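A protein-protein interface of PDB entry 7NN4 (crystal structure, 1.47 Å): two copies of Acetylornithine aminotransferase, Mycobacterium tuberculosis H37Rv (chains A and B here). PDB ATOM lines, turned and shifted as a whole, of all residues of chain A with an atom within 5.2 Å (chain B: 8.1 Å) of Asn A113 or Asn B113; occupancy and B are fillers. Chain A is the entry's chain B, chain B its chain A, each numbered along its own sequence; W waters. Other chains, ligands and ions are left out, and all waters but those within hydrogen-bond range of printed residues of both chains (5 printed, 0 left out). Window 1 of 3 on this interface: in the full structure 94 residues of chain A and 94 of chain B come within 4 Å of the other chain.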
ATOM      1  N   PHE A 111      -1.628  -4.675 -23.330  1.00  0.00           N
ATOM      2  CA  PHE A 111      -0.675  -5.748 -23.080  1.00  0.00           C
ATOM      3  C   PHE A 111      -0.906  -6.948 -23.989  1.00  0.00           C
ATOM      4  O   PHE A 111      -2.033  -7.261 -24.383  1.00  0.00           O
ATOM      5  CB  PHE A 111      -0.733  -6.208 -21.623  1.00  0.00           C
ATOM      6  CG  PHE A 111      -0.185  -5.204 -20.654  1.00  0.00           C
ATOM      7  CD1 PHE A 111       1.130  -4.787 -20.735  1.00  0.00           C
ATOM      8  CD2 PHE A 111      -0.990  -4.693 -19.639  1.00  0.00           C
ATOM      9  CE1 PHE A 111       1.638  -3.872 -19.847  1.00  0.00           C
ATOM     10  CE2 PHE A 111      -0.471  -3.774 -18.739  1.00  0.00           C
ATOM     11  CZ  PHE A 111       0.845  -3.365 -18.850  1.00  0.00           C
ATOM     12  N   CYS A 112       0.188  -7.627 -24.309  1.00  0.00           N
ATOM     13  CA  CYS A 112       0.156  -8.831 -25.137  1.00  0.00           C
ATOM     14  C   CYS A 112       1.344  -9.693 -24.729  1.00  0.00           C
ATOM     15  O   CYS A 112       1.905  -9.504 -23.649  1.00  0.00           O
ATOM     16  CB  CYS A 112       0.150  -8.453 -26.626  1.00  0.00           C
ATOM     17  SG  CYS A 112       1.499  -7.368 -27.104  1.00  0.00           S
ATOM     18  N   ASN A 113       1.765 -10.609 -25.609  1.00  0.00           N
ATOM     19  CA  ASN A 113       2.736 -11.619 -25.199  1.00  0.00           C
ATOM     20  C   ASN A 113       4.084 -11.528 -25.882  1.00  0.00           C
ATOM     21  O   ASN A 113       4.969 -12.311 -25.530  1.00  0.00           O
ATOM     22  CB  ASN A 113       2.211 -13.026 -25.501  1.00  0.00           C
ATOM     23  CG  ASN A 113       0.918 -13.308 -24.819  1.00  0.00           C
ATOM     24  OD1 ASN A 113       0.879 -13.480 -23.611  1.00  0.00           O
ATOM     25  ND2 ASN A 113      -0.167 -13.349 -25.592  1.00  0.00           N
ATOM     26  N   SER A 114       4.262 -10.656 -26.865  1.00  0.00           N
ATOM     27  CA  SER A 114       5.461 -10.742 -27.686  1.00  0.00           C
ATOM     28  C   SER A 114       5.660  -9.434 -28.429  1.00  0.00           C
ATOM     29  O   SER A 114       4.770  -8.585 -28.493  1.00  0.00           O
ATOM     30  CB  SER A 114       5.342 -11.881 -28.702  1.00  0.00           C
ATOM     31  OG  SER A 114       4.298 -11.618 -29.630  1.00  0.00           O
ATOM     32  N   GLY A 115       6.843  -9.308 -29.036  1.00  0.00           N
ATOM     33  CA  GLY A 115       7.126  -8.156 -29.872  1.00  0.00           C
ATOM     34  C   GLY A 115       6.265  -8.129 -31.117  1.00  0.00           C
ATOM     35  O   GLY A 115       5.731  -7.081 -31.490  1.00  0.00           O
ATOM     36  N   GLU A 117       3.282  -9.412 -31.439  1.00  0.00           N
ATOM     37  CA  GLU A 117       1.927  -9.035 -31.039  1.00  0.00           C
ATOM     38  C   GLU A 117       1.835  -7.553 -30.725  1.00  0.00           C
ATOM     39  O   GLU A 117       0.815  -6.920 -31.018  1.00  0.00           O
ATOM     40  CB  GLU A 117       1.446  -9.866 -29.848  1.00  0.00           C
ATOM     41  CG  GLU A 117       1.065 -11.268 -30.257  1.00  0.00           C
ATOM     42  CD  GLU A 117       0.418 -12.043 -29.133  1.00  0.00           C
ATOM     43  OE1 GLU A 117       0.518 -11.611 -27.969  1.00  0.00           O
ATOM     44  OE2 GLU A 117      -0.211 -13.082 -29.416  1.00  0.00           O
ATOM     45  N   PRO A 262       7.139 -14.107 -20.721  1.00  0.00           N
ATOM     46  CA  PRO A 262       6.596 -13.552 -21.977  1.00  0.00           C
ATOM     47  C   PRO A 262       5.600 -12.438 -21.699  1.00  0.00           C
ATOM     48  O   PRO A 262       4.559 -12.664 -21.086  1.00  0.00           O
ATOM     49  CB  PRO A 262       5.906 -14.752 -22.643  1.00  0.00           C
ATOM     50  CG  PRO A 262       6.411 -15.968 -21.913  1.00  0.00           C
ATOM     51  CD  PRO A 262       6.812 -15.531 -20.531  1.00  0.00           C
ATOM     52  N   ILE A 263       5.916 -11.241 -22.187  1.00  0.00           N
ATOM     53  CA  ILE A 263       5.021 -10.089 -22.083  1.00  0.00           C
ATOM     54  C   ILE A 263       5.477  -9.036 -23.079  1.00  0.00           C
ATOM     55  O   ILE A 263       6.678  -8.851 -23.311  1.00  0.00           O
ATOM     56  CB  ILE A 263       4.919  -9.547 -20.633  1.00  0.00           C
ATOM     57  CG1 ILE A 263       4.015  -8.319 -20.568  1.00  0.00           C
ATOM     58  CG2 ILE A 263       6.298  -9.197 -20.064  1.00  0.00           C
ATOM     59  CD1 ILE A 263       3.541  -7.998 -19.130  1.00  0.00           C
ATOM     60  N   GLY A 264       4.501  -8.370 -23.697  1.00  0.00           N
ATOM     61  CA  GLY A 264       4.771  -7.255 -24.576  1.00  0.00           C
ATOM     62  C   GLY A 264       3.757  -6.163 -24.303  1.00  0.00           C
ATOM     63  O   GLY A 264       2.761  -6.396 -23.627  1.00  0.00           O
ATOM     64  N   SER A 283      -6.147  -9.976 -26.365  1.00  0.00           N
ATOM     65  CA  SER A 283      -5.241 -11.118 -26.275  1.00  0.00           C
ATOM     66  C   SER A 283      -5.540 -11.826 -24.968  1.00  0.00           C
ATOM     67  O   SER A 283      -5.479 -11.193 -23.916  1.00  0.00           O
ATOM     68  CB  SER A 283      -3.791 -10.641 -26.208  1.00  0.00           C
ATOM     69  OG  SER A 283      -2.914 -11.741 -26.372  1.00  0.00           O
ATOM     70  N   PHE A 285      -4.030 -13.898 -22.873  1.00  0.00           N
ATOM     71  CA  PHE A 285      -3.053 -13.839 -21.794  1.00  0.00           C
ATOM     72  C   PHE A 285      -2.573 -12.421 -21.504  1.00  0.00           C
ATOM     73  O   PHE A 285      -1.811 -12.234 -20.552  1.00  0.00           O
ATOM     74  CB  PHE A 285      -1.804 -14.632 -22.183  1.00  0.00           C
ATOM     75  CG  PHE A 285      -2.020 -16.112 -22.398  1.00  0.00           C
ATOM     76  CD1 PHE A 285      -2.768 -16.876 -21.515  1.00  0.00           C
ATOM     77  CD2 PHE A 285      -1.405 -16.746 -23.470  1.00  0.00           C
ATOM     78  CE1 PHE A 285      -2.915 -18.245 -21.711  1.00  0.00           C
ATOM     79  CE2 PHE A 285      -1.545 -18.101 -23.680  1.00  0.00           C
ATOM     80  CZ  PHE A 285      -2.298 -18.865 -22.799  1.00  0.00           C
ATOM     81  N   GLY A 286      -2.977 -11.428 -22.291  1.00  0.00           N
ATOM     82  CA  GLY A 286      -2.461 -10.079 -22.115  1.00  0.00           C
ATOM     83  C   GLY A 286      -2.652  -9.485 -20.731  1.00  0.00           C
ATOM     84  O   GLY A 286      -3.765  -9.458 -20.197  1.00  0.00           O
ATOM     85  N   ASN A 288      -1.574 -10.557 -17.851  1.00  0.00           N
ATOM     86  CA  ASN A 288      -1.862 -11.495 -16.784  1.00  0.00           C
ATOM     87  C   ASN A 288      -0.994 -11.201 -15.555  1.00  0.00           C
ATOM     88  O   ASN A 288       0.137 -10.707 -15.674  1.00  0.00           O
ATOM     89  CB  ASN A 288      -1.665 -12.932 -17.250  1.00  0.00           C
ATOM     90  CG  ASN A 288      -0.203 -13.298 -17.412  1.00  0.00           C
ATOM     91  OD1 ASN A 288       0.470 -13.697 -16.449  1.00  0.00           O
ATOM     92  ND2 ASN A 288       0.287 -13.206 -18.632  1.00  0.00           N
ATOM     93  N   PHE B 110       6.149 -26.434 -33.116  1.00  0.00           N
ATOM     94  CA  PHE B 110       6.653 -25.067 -33.002  1.00  0.00           C
ATOM     95  C   PHE B 110       5.948 -24.403 -31.831  1.00  0.00           C
ATOM     96  O   PHE B 110       4.716 -24.443 -31.741  1.00  0.00           O
ATOM     97  CB  PHE B 110       6.367 -24.278 -34.282  1.00  0.00           C
ATOM     98  CG  PHE B 110       6.546 -22.797 -34.119  1.00  0.00           C
ATOM     99  CD1 PHE B 110       7.818 -22.254 -34.090  1.00  0.00           C
ATOM    100  CD2 PHE B 110       5.454 -21.958 -33.983  1.00  0.00           C
ATOM    101  CE1 PHE B 110       8.004 -20.888 -33.901  1.00  0.00           C
ATOM    102  CE2 PHE B 110       5.626 -20.599 -33.809  1.00  0.00           C
ATOM    103  CZ  PHE B 110       6.909 -20.064 -33.777  1.00  0.00           C
ATOM    104  N   PHE B 111       6.714 -23.793 -30.926  1.00  0.00           N
ATOM    105  CA  PHE B 111       6.124 -23.125 -29.774  1.00  0.00           C
ATOM    106  C   PHE B 111       6.042 -21.620 -29.980  1.00  0.00           C
ATOM    107  O   PHE B 111       6.888 -21.007 -30.634  1.00  0.00           O
ATOM    108  CB  PHE B 111       6.938 -23.402 -28.514  1.00  0.00           C
ATOM    109  CG  PHE B 111       6.834 -24.815 -28.037  1.00  0.00           C
ATOM    110  CD1 PHE B 111       5.613 -25.329 -27.640  1.00  0.00           C
ATOM    111  CD2 PHE B 111       7.954 -25.632 -27.991  1.00  0.00           C
ATOM    112  CE1 PHE B 111       5.502 -26.639 -27.191  1.00  0.00           C
ATOM    113  CE2 PHE B 111       7.845 -26.954 -27.551  1.00  0.00           C
ATOM    114  CZ  PHE B 111       6.621 -27.446 -27.147  1.00  0.00           C
ATOM    115  N   CYS B 112       5.029 -21.027 -29.364  1.00  0.00           N
ATOM    116  CA  CYS B 112       4.820 -19.584 -29.397  1.00  0.00           C
ATOM    117  C   CYS B 112       4.126 -19.198 -28.093  1.00  0.00           C
ATOM    118  O   CYS B 112       4.167 -19.946 -27.112  1.00  0.00           O
ATOM    119  CB  CYS B 112       4.060 -19.161 -30.664  1.00  0.00           C
ATOM    120  SG  CYS B 112       2.529 -20.061 -30.903  1.00  0.00           S
ATOM    121  N   ASN B 113       3.455 -18.046 -28.083  1.00  0.00           N
ATOM    122  CA  ASN B 113       2.953 -17.487 -26.830  1.00  0.00           C
ATOM    123  C   ASN B 113       1.447 -17.465 -26.704  1.00  0.00           C
ATOM    124  O   ASN B 113       0.951 -17.226 -25.598  1.00  0.00           O
ATOM    125  CB  ASN B 113       3.427 -16.041 -26.667  1.00  0.00           C
ATOM    126  CG  ASN B 113       4.908 -15.923 -26.687  1.00  0.00           C
ATOM    127  OD1 ASN B 113       5.591 -16.346 -25.749  1.00  0.00           O
ATOM    128  ND2 ASN B 113       5.431 -15.371 -27.766  1.00  0.00           N
ATOM    129  N   SER B 114       0.709 -17.699 -27.781  1.00  0.00           N
ATOM    130  CA  SER B 114      -0.713 -17.396 -27.777  1.00  0.00           C
ATOM    131  C   SER B 114      -1.401 -18.207 -28.867  1.00  0.00           C
ATOM    132  O   SER B 114      -0.759 -18.763 -29.762  1.00  0.00           O
ATOM    133  CB  SER B 114      -0.952 -15.907 -28.033  1.00  0.00           C
ATOM    134  OG  SER B 114      -0.550 -15.599 -29.368  1.00  0.00           O
ATOM    135  N   GLY B 115      -2.733 -18.236 -28.785  1.00  0.00           N
ATOM    136  CA  GLY B 115      -3.520 -18.868 -29.831  1.00  0.00           C
ATOM    137  C   GLY B 115      -3.419 -18.147 -31.160  1.00  0.00           C
ATOM    138  O   GLY B 115      -3.288 -18.783 -32.216  1.00  0.00           O
ATOM    139  N   ALA B 116      -3.472 -16.815 -31.136  1.00  0.00           N
ATOM    140  CA  ALA B 116      -3.276 -16.071 -32.376  1.00  0.00           C
ATOM    141  C   ALA B 116      -1.941 -16.417 -33.014  1.00  0.00           C
ATOM    142  O   ALA B 116      -1.874 -16.656 -34.226  1.00  0.00           O
ATOM    143  CB  ALA B 116      -3.399 -14.571 -32.128  1.00  0.00           C
ATOM    144  N   GLU B 117      -0.867 -16.468 -32.214  1.00  0.00           N
ATOM    145  CA  GLU B 117       0.438 -16.776 -32.794  1.00  0.00           C
ATOM    146  C   GLU B 117       0.506 -18.202 -33.308  1.00  0.00           C
ATOM    147  O   GLU B 117       1.187 -18.454 -34.309  1.00  0.00           O
ATOM    148  CB  GLU B 117       1.564 -16.527 -31.783  1.00  0.00           C
ATOM    149  CG  GLU B 117       1.907 -15.052 -31.572  1.00  0.00           C
ATOM    150  CD  GLU B 117       3.097 -14.864 -30.651  1.00  0.00           C
ATOM    151  OE1 GLU B 117       3.475 -15.806 -29.934  1.00  0.00           O
ATOM    152  OE2 GLU B 117       3.677 -13.768 -30.658  1.00  0.00           O
ATOM    153  N   ALA B 118      -0.172 -19.147 -32.636  1.00  0.00           N
ATOM    154  CA  ALA B 118      -0.185 -20.521 -33.125  1.00  0.00           C
ATOM    155  C   ALA B 118      -0.863 -20.592 -34.484  1.00  0.00           C
ATOM    156  O   ALA B 118      -0.359 -21.249 -35.405  1.00  0.00           O
ATOM    157  CB  ALA B 118      -0.873 -21.437 -32.106  1.00  0.00           C
ATOM    158  N   LEU B 253      -2.750 -25.102 -30.428  1.00  0.00           N
ATOM    159  CA  LEU B 253      -3.107 -25.130 -28.991  1.00  0.00           C
ATOM    160  C   LEU B 253      -2.588 -23.851 -28.332  1.00  0.00           C
ATOM    161  O   LEU B 253      -1.646 -23.311 -28.819  1.00  0.00           O
ATOM    162  CB  LEU B 253      -2.366 -26.278 -28.306  1.00  0.00           C
ATOM    163  CG  LEU B 253      -2.727 -27.713 -28.622  1.00  0.00           C
ATOM    164  CD1 LEU B 253      -1.718 -28.609 -27.915  1.00  0.00           C
ATOM    165  CD2 LEU B 253      -4.105 -28.031 -28.110  1.00  0.00           C
ATOM    166  N   ALA B 254      -3.264 -23.453 -27.270  1.00  0.00           N
ATOM    167  CA  ALA B 254      -2.883 -22.325 -26.402  1.00  0.00           C
ATOM    168  C   ALA B 254      -3.825 -22.369 -25.196  1.00  0.00           C
ATOM    169  O   ALA B 254      -4.140 -23.452 -24.746  1.00  0.00           O
ATOM    170  CB  ALA B 254      -2.924 -20.983 -27.110  1.00  0.00           C
ATOM    171  N1  LLP B 255      -8.546 -19.718 -31.276  1.00  0.00           N
ATOM    172  C2  LLP B 255      -9.505 -20.074 -30.448  1.00  0.00           C
ATOM    173  C2' LLP B 255     -10.401 -21.204 -30.824  1.00  0.00           C
ATOM    174  C3  LLP B 255      -9.651 -19.448 -29.232  1.00  0.00           C
ATOM    175  O3  LLP B 255     -10.645 -19.857 -28.453  1.00  0.00           O
ATOM    176  C4  LLP B 255      -8.779 -18.430 -28.850  1.00  0.00           C
ATOM    177  C4' LLP B 255      -8.921 -17.867 -27.504  1.00  0.00           C
ATOM    178  C5  LLP B 255      -7.790 -18.038 -29.757  1.00  0.00           C
ATOM    179  C6  LLP B 255      -7.729 -18.710 -30.942  1.00  0.00           C
ATOM    180  C5' LLP B 255      -6.889 -16.863 -29.523  1.00  0.00           C
ATOM    181  OP4 LLP B 255      -5.902 -17.031 -28.489  1.00  0.00           O
ATOM    182  P   LLP B 255      -5.136 -15.769 -27.935  1.00  0.00           P
ATOM    183  OP1 LLP B 255      -6.154 -14.927 -27.322  1.00  0.00           O
ATOM    184  OP2 LLP B 255      -4.165 -16.362 -26.991  1.00  0.00           O
ATOM    185  OP3 LLP B 255      -4.517 -15.113 -29.094  1.00  0.00           O
ATOM    186  N   LLP B 255      -4.252 -21.200 -24.748  1.00  0.00           N
ATOM    187  CA  LLP B 255      -5.147 -21.056 -23.568  1.00  0.00           C
ATOM    188  CB  LLP B 255      -6.620 -21.207 -23.944  1.00  0.00           C
ATOM    189  CG  LLP B 255      -7.163 -19.993 -24.670  1.00  0.00           C
ATOM    190  CD  LLP B 255      -8.676 -19.865 -24.698  1.00  0.00           C
ATOM    191  CE  LLP B 255      -9.133 -18.492 -25.187  1.00  0.00           C
ATOM    192  NZ  LLP B 255      -9.523 -18.524 -26.597  1.00  0.00           N
ATOM    193  C   LLP B 255      -4.702 -21.932 -22.394  1.00  0.00           C
ATOM    194  O   LLP B 255      -3.776 -21.544 -21.734  1.00  0.00           O
ATOM    195  N   LEU B 257      -2.973 -24.658 -22.242  1.00  0.00           N
ATOM    196  CA  LEU B 257      -1.708 -25.401 -22.424  1.00  0.00           C
ATOM    197  C   LEU B 257      -0.722 -25.188 -21.273  1.00  0.00           C
ATOM    198  O   LEU B 257      -0.123 -26.130 -20.876  1.00  0.00           O
ATOM    199  CB  LEU B 257      -1.078 -24.998 -23.757  1.00  0.00           C
ATOM    200  CG  LEU B 257       0.236 -25.696 -24.092  1.00  0.00           C
ATOM    201  CD1 LEU B 257       0.080 -27.202 -24.070  1.00  0.00           C
ATOM    202  CD2 LEU B 257       0.772 -25.243 -25.447  1.00  0.00           C
ATOM    203  N   GLY B 260      -2.213 -21.386 -17.380  1.00  0.00           N
ATOM    204  CA  GLY B 260      -2.207 -19.989 -17.003  1.00  0.00           C
ATOM    205  C   GLY B 260      -0.972 -19.267 -17.511  1.00  0.00           C
ATOM    206  O   GLY B 260      -1.040 -18.080 -17.824  1.00  0.00           O
ATOM    207  N   LEU B 261       0.144 -19.958 -17.610  1.00  0.00           N
ATOM    208  CA  LEU B 261       1.339 -19.307 -18.145  1.00  0.00           C
ATOM    209  C   LEU B 261       1.201 -19.171 -19.663  1.00  0.00           C
ATOM    210  O   LEU B 261       0.664 -20.067 -20.312  1.00  0.00           O
ATOM    211  CB  LEU B 261       2.583 -20.139 -17.817  1.00  0.00           C
ATOM    212  CG  LEU B 261       3.205 -19.982 -16.418  1.00  0.00           C
ATOM    213  CD1 LEU B 261       3.752 -18.577 -16.217  1.00  0.00           C
ATOM    214  CD2 LEU B 261       2.247 -20.352 -15.290  1.00  0.00           C
ATOM    215  N   PRO B 262       1.658 -18.069 -20.258  1.00  0.00           N
ATOM    216  CA  PRO B 262       1.453 -17.881 -21.708  1.00  0.00           C
ATOM    217  C   PRO B 262       2.297 -18.844 -22.530  1.00  0.00           C
ATOM    218  O   PRO B 262       3.530 -18.793 -22.496  1.00  0.00           O
ATOM    219  CB  PRO B 262       1.876 -16.423 -21.950  1.00  0.00           C
ATOM    220  CG  PRO B 262       1.911 -15.781 -20.605  1.00  0.00           C
ATOM    221  CD  PRO B 262       2.229 -16.870 -19.619  1.00  0.00           C
ATOM    222  N   ILE B 263       1.627 -19.697 -23.304  1.00  0.00           N
ATOM    223  CA  ILE B 263       2.302 -20.600 -24.228  1.00  0.00           C
ATOM    224  C   ILE B 263       1.268 -21.113 -25.222  1.00  0.00           C
ATOM    225  O   ILE B 263       0.106 -21.331 -24.869  1.00  0.00           O
ATOM    226  CB  ILE B 263       3.031 -21.746 -23.481  1.00  0.00           C
ATOM    227  CG1 ILE B 263       3.683 -22.717 -24.463  1.00  0.00           C
ATOM    228  CG2 ILE B 263       2.063 -22.498 -22.550  1.00  0.00           C
ATOM    229  CD1 ILE B 263       4.663 -23.694 -23.799  1.00  0.00           C
ATOM    230  N   GLY B 264       1.703 -21.257 -26.474  1.00  0.00           N
ATOM    231  CA  GLY B 264       0.898 -21.859 -27.517  1.00  0.00           C
ATOM    232  C   GLY B 264       1.765 -22.800 -28.328  1.00  0.00           C
ATOM    233  O   GLY B 264       2.993 -22.800 -28.204  1.00  0.00           O
ATOM    234  N   ALA B 265       1.118 -23.607 -29.167  1.00  0.00           N
ATOM    235  CA  ALA B 265       1.890 -24.545 -29.969  1.00  0.00           C
ATOM    236  C   ALA B 265       1.198 -24.793 -31.293  1.00  0.00           C
ATOM    237  O   ALA B 265      -0.037 -24.785 -31.382  1.00  0.00           O
ATOM    238  CB  ALA B 265       2.114 -25.890 -29.253  1.00  0.00           C
ATOM    239  N   GLY B 282       9.801 -17.943 -36.373  1.00  0.00           N
ATOM    240  CA  GLY B 282      10.340 -17.950 -35.019  1.00  0.00           C
ATOM    241  C   GLY B 282       9.508 -17.057 -34.123  1.00  0.00           C
ATOM    242  O   GLY B 282       8.654 -16.296 -34.584  1.00  0.00           O
ATOM    243  N   SER B 283       9.776 -17.175 -32.824  1.00  0.00           N
ATOM    244  CA  SER B 283       9.184 -16.331 -31.782  1.00  0.00           C
ATOM    245  C   SER B 283      10.185 -16.294 -30.642  1.00  0.00           C
ATOM    246  O   SER B 283      10.585 -17.351 -30.153  1.00  0.00           O
ATOM    247  CB  SER B 283       7.860 -16.915 -31.279  1.00  0.00           C
ATOM    248  OG  SER B 283       7.239 -16.019 -30.364  1.00  0.00           O
ATOM    249  N   THR B 284      10.596 -15.092 -30.221  1.00  0.00           N
ATOM    250  CA  THR B 284      11.675 -14.986 -29.238  1.00  0.00           C
ATOM    251  C   THR B 284      11.428 -15.846 -28.000  1.00  0.00           C
ATOM    252  O   THR B 284      12.307 -16.613 -27.580  1.00  0.00           O
ATOM    253  CB  THR B 284      11.864 -13.532 -28.824  1.00  0.00           C
ATOM    254  OG1 THR B 284      12.302 -12.775 -29.957  1.00  0.00           O
ATOM    255  CG2 THR B 284      12.945 -13.432 -27.748  1.00  0.00           C
ATOM    256  N   PHE B 285      10.259 -15.701 -27.379  1.00  0.00           N
ATOM    257  CA  PHE B 285       9.947 -16.418 -26.147  1.00  0.00           C
ATOM    258  C   PHE B 285       9.495 -17.857 -26.387  1.00  0.00           C
ATOM    259  O   PHE B 285       9.224 -18.559 -25.407  1.00  0.00           O
ATOM    260  CB  PHE B 285       8.789 -15.744 -25.400  1.00  0.00           C
ATOM    261  CG  PHE B 285       9.028 -14.315 -24.972  1.00  0.00           C
ATOM    262  CD1 PHE B 285      10.193 -13.917 -24.326  1.00  0.00           C
ATOM    263  CD2 PHE B 285       8.026 -13.378 -25.173  1.00  0.00           C
ATOM    264  CE1 PHE B 285      10.352 -12.586 -23.901  1.00  0.00           C
ATOM    265  CE2 PHE B 285       8.169 -12.056 -24.765  1.00  0.00           C
ATOM    266  CZ  PHE B 285       9.341 -11.657 -24.120  1.00  0.00           C
ATOM    267  N   GLY B 286       9.355 -18.295 -27.638  1.00  0.00           N
ATOM    268  CA  GLY B 286       8.735 -19.592 -27.884  1.00  0.00           C
ATOM    269  C   GLY B 286       9.488 -20.738 -27.241  1.00  0.00           C
ATOM    270  O   GLY B 286      10.711 -20.826 -27.369  1.00  0.00           O
ATOM    271  N   GLY B 287       8.773 -21.615 -26.540  1.00  0.00           N
ATOM    272  CA  GLY B 287       9.435 -22.780 -25.987  1.00  0.00           C
ATOM    273  C   GLY B 287      10.296 -22.511 -24.780  1.00  0.00           C
ATOM    274  O   GLY B 287      11.087 -23.378 -24.394  1.00  0.00           O
ATOM    275  N   ASN B 288      10.155 -21.348 -24.153  1.00  0.00           N
ATOM    276  CA  ASN B 288      11.040 -21.017 -23.049  1.00  0.00           C
ATOM    277  C   ASN B 288      10.855 -21.997 -21.891  1.00  0.00           C
ATOM    278  O   ASN B 288       9.773 -22.563 -21.697  1.00  0.00           O
ATOM    279  CB  ASN B 288      10.831 -19.579 -22.580  1.00  0.00           C
ATOM    280  CG  ASN B 288       9.544 -19.400 -21.801  1.00  0.00           C
ATOM    281  OD1 ASN B 288       9.498 -19.611 -20.581  1.00  0.00           O
ATOM    282  ND2 ASN B 288       8.484 -18.986 -22.496  1.00  0.00           N
ATOM    283  N   CYS B 291       7.694 -21.498 -19.130  1.00  0.00           N
ATOM    284  CA  CYS B 291       6.330 -21.778 -19.574  1.00  0.00           C
ATOM    285  C   CYS B 291       6.187 -23.227 -20.002  1.00  0.00           C
ATOM    286  O   CYS B 291       5.143 -23.845 -19.770  1.00  0.00           O
ATOM    287  CB  CYS B 291       5.987 -20.865 -20.742  1.00  0.00           C
ATOM    288  SG  CYS B 291       5.882 -19.141 -20.173  1.00  0.00           S
HETATM  289  O   HOH W   1       6.062 -13.812 -31.641  1.00  0.00           O
HETATM  290  O   HOH W   2      -1.995 -15.571 -18.597  1.00  0.00           O
HETATM  291  O   HOH W   3      -2.951 -14.460 -25.447  1.00  0.00           O
HETATM  292  O   HOH W   4       0.430 -16.502 -16.167  1.00  0.00           O
HETATM  293  O   HOH W   5      -2.793 -12.948 -28.831  1.00  0.00           O
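The side-chain carboxylate of Glu A117 is in hydrogen-bond range of the side-chain hydroxyl of Ser B114 (2.5 Å). The side-chain hydroxyl (OG) of Ser A114 is in hydrogen-bond range of the side-chain carboxylate (OE2) of Glu B117 (2.5 Å).
The side-chain sulfur (SG) of Cys B112 lies within hydrogen-bond range of the backbone carbonyl oxygen (O) of Ser B114 (3.7 Å). The backbone NH of Asn B113 sits at hydrogen-bond distance from the side-chain carboxylate of Glu B117 (2.9 Å). The side-chain hydroxyl of Ser B283 sits at hydrogen-bond distance from the side-chain amide nitrogen of Asn B113, at 3.2 Å. OP2 of LLP B255 is in hydrogen-bond range of N of Gly B115 (3.0 Å). O of Pro B262 is in hydrogen-bond range of SG of Cys B291, 3.3 Å away. The side-chain amide nitrogen of Asn A113 lies within hydrogen-bond range of the side-chain hydroxyl of Ser A283.
Asn A113 touches Asn B113. CB of Pro B262 touches OD1 of Asn A113, 3.5 Å away. Ser A114 touches Asn B113. Phe B285 touches Pro A262. CG of Pro A262 touches SG of Cys B291, at 3.7 Å. Phe B285 touches Ile A263 (CE2 to N, 3.5 Å). CD2 of Phe A285 touches O of Asn B113, 3.2 Å away. CA of Pro B262 touches CD2 of Phe A285, at 3.5 Å. Phe A285 touches Ile B263. Pro B262 touches Asn A288 (CG to ND2, 3.6 Å).
No residue of chain B comes within 4 Å of Cys A112. Asn A113 touches just these residues of chain B: Asn B113 (3.5 Å), Ser B114 (3.6 Å), Pro B262 (3.5 Å) and Phe B285 (3.3 Å). Ser A114 touches just these residues of chain B: Asn B113 and Glu B117. Of the printed residues of chain B, Glu A117 touches Ser B114 and Glu B117. Of the printed residues of chain B, Ser A283 touches LLP B255 (3.9 Å). Cys B112 touches none of the printed residues of chain A. Asn B113 touches just these residues of chain A: Asn A113, Ser A114, Pro A262 and Phe A285. Of the printed residues of chain A, Glu B117 touches Ser A114 (2.5 Å) and Glu A117 (3.6 Å). Ala B254 touches none of the printed residues of chain A. Of the printed residues of chain A, LLP B255 touches Ser A283 and Phe A285.
Printed residues of chain B that touch a printed residue of chain A: Asn B113, Ser B114, Glu B117, LLP B255, Pro B262, Ile B263, Phe B285, Asn B288 and Cys B291. Hydrophobic or aromatic side chains of chain A within 4 Å of the printed part of chain B: Pro A262 and Phe A285.
Asn A113 touches its own counterpart, Asn B113. Asn A113 touches Pro B262, and with the chains exchanged Pro A262 touches Asn B113. Ser A114 touches Glu B117, and with the chains exchanged Glu A117 touches Ser B114. Ile A263 touches Phe B285, and with the chains exchanged Phe A285 touches Ile B263. 13 positions are printed for both chains. Of the 19 pairs that touch across the chains among the printed residues, 16 have their exchanged pair printed and touching as well.
Water W1 lies within hydrogen-bond range of the side-chain carboxylate (OE2) of Glu B117 (2.6 Å), the side-chain hydroxyl (OG) of Ser B283 (2.8 Å) and the side-chain hydroxyl (OG) of Ser A114 (3.5 Å). Water W5 lies within hydrogen-bond range of the side-chain carboxylate of Glu A117 (2.7 Å), the side-chain hydroxyl of Ser A283 (2.7 Å) and OP3 of LLP B255 (2.8 Å). Water W4 lies within hydrogen-bond range of the backbone carbonyl oxygen of Gly B260 and the side-chain amide oxygen of Asn A288. Water W3 lies within hydrogen-bond range of OP2 of LLP B255, N of Phe A285, OG of Ser A283 and ND2 of Asn A113. Water W2 bridges the backbone carbonyl oxygen (O) of Gly B260 and the side-chain amide nitrogen (ND2) of Asn A288.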
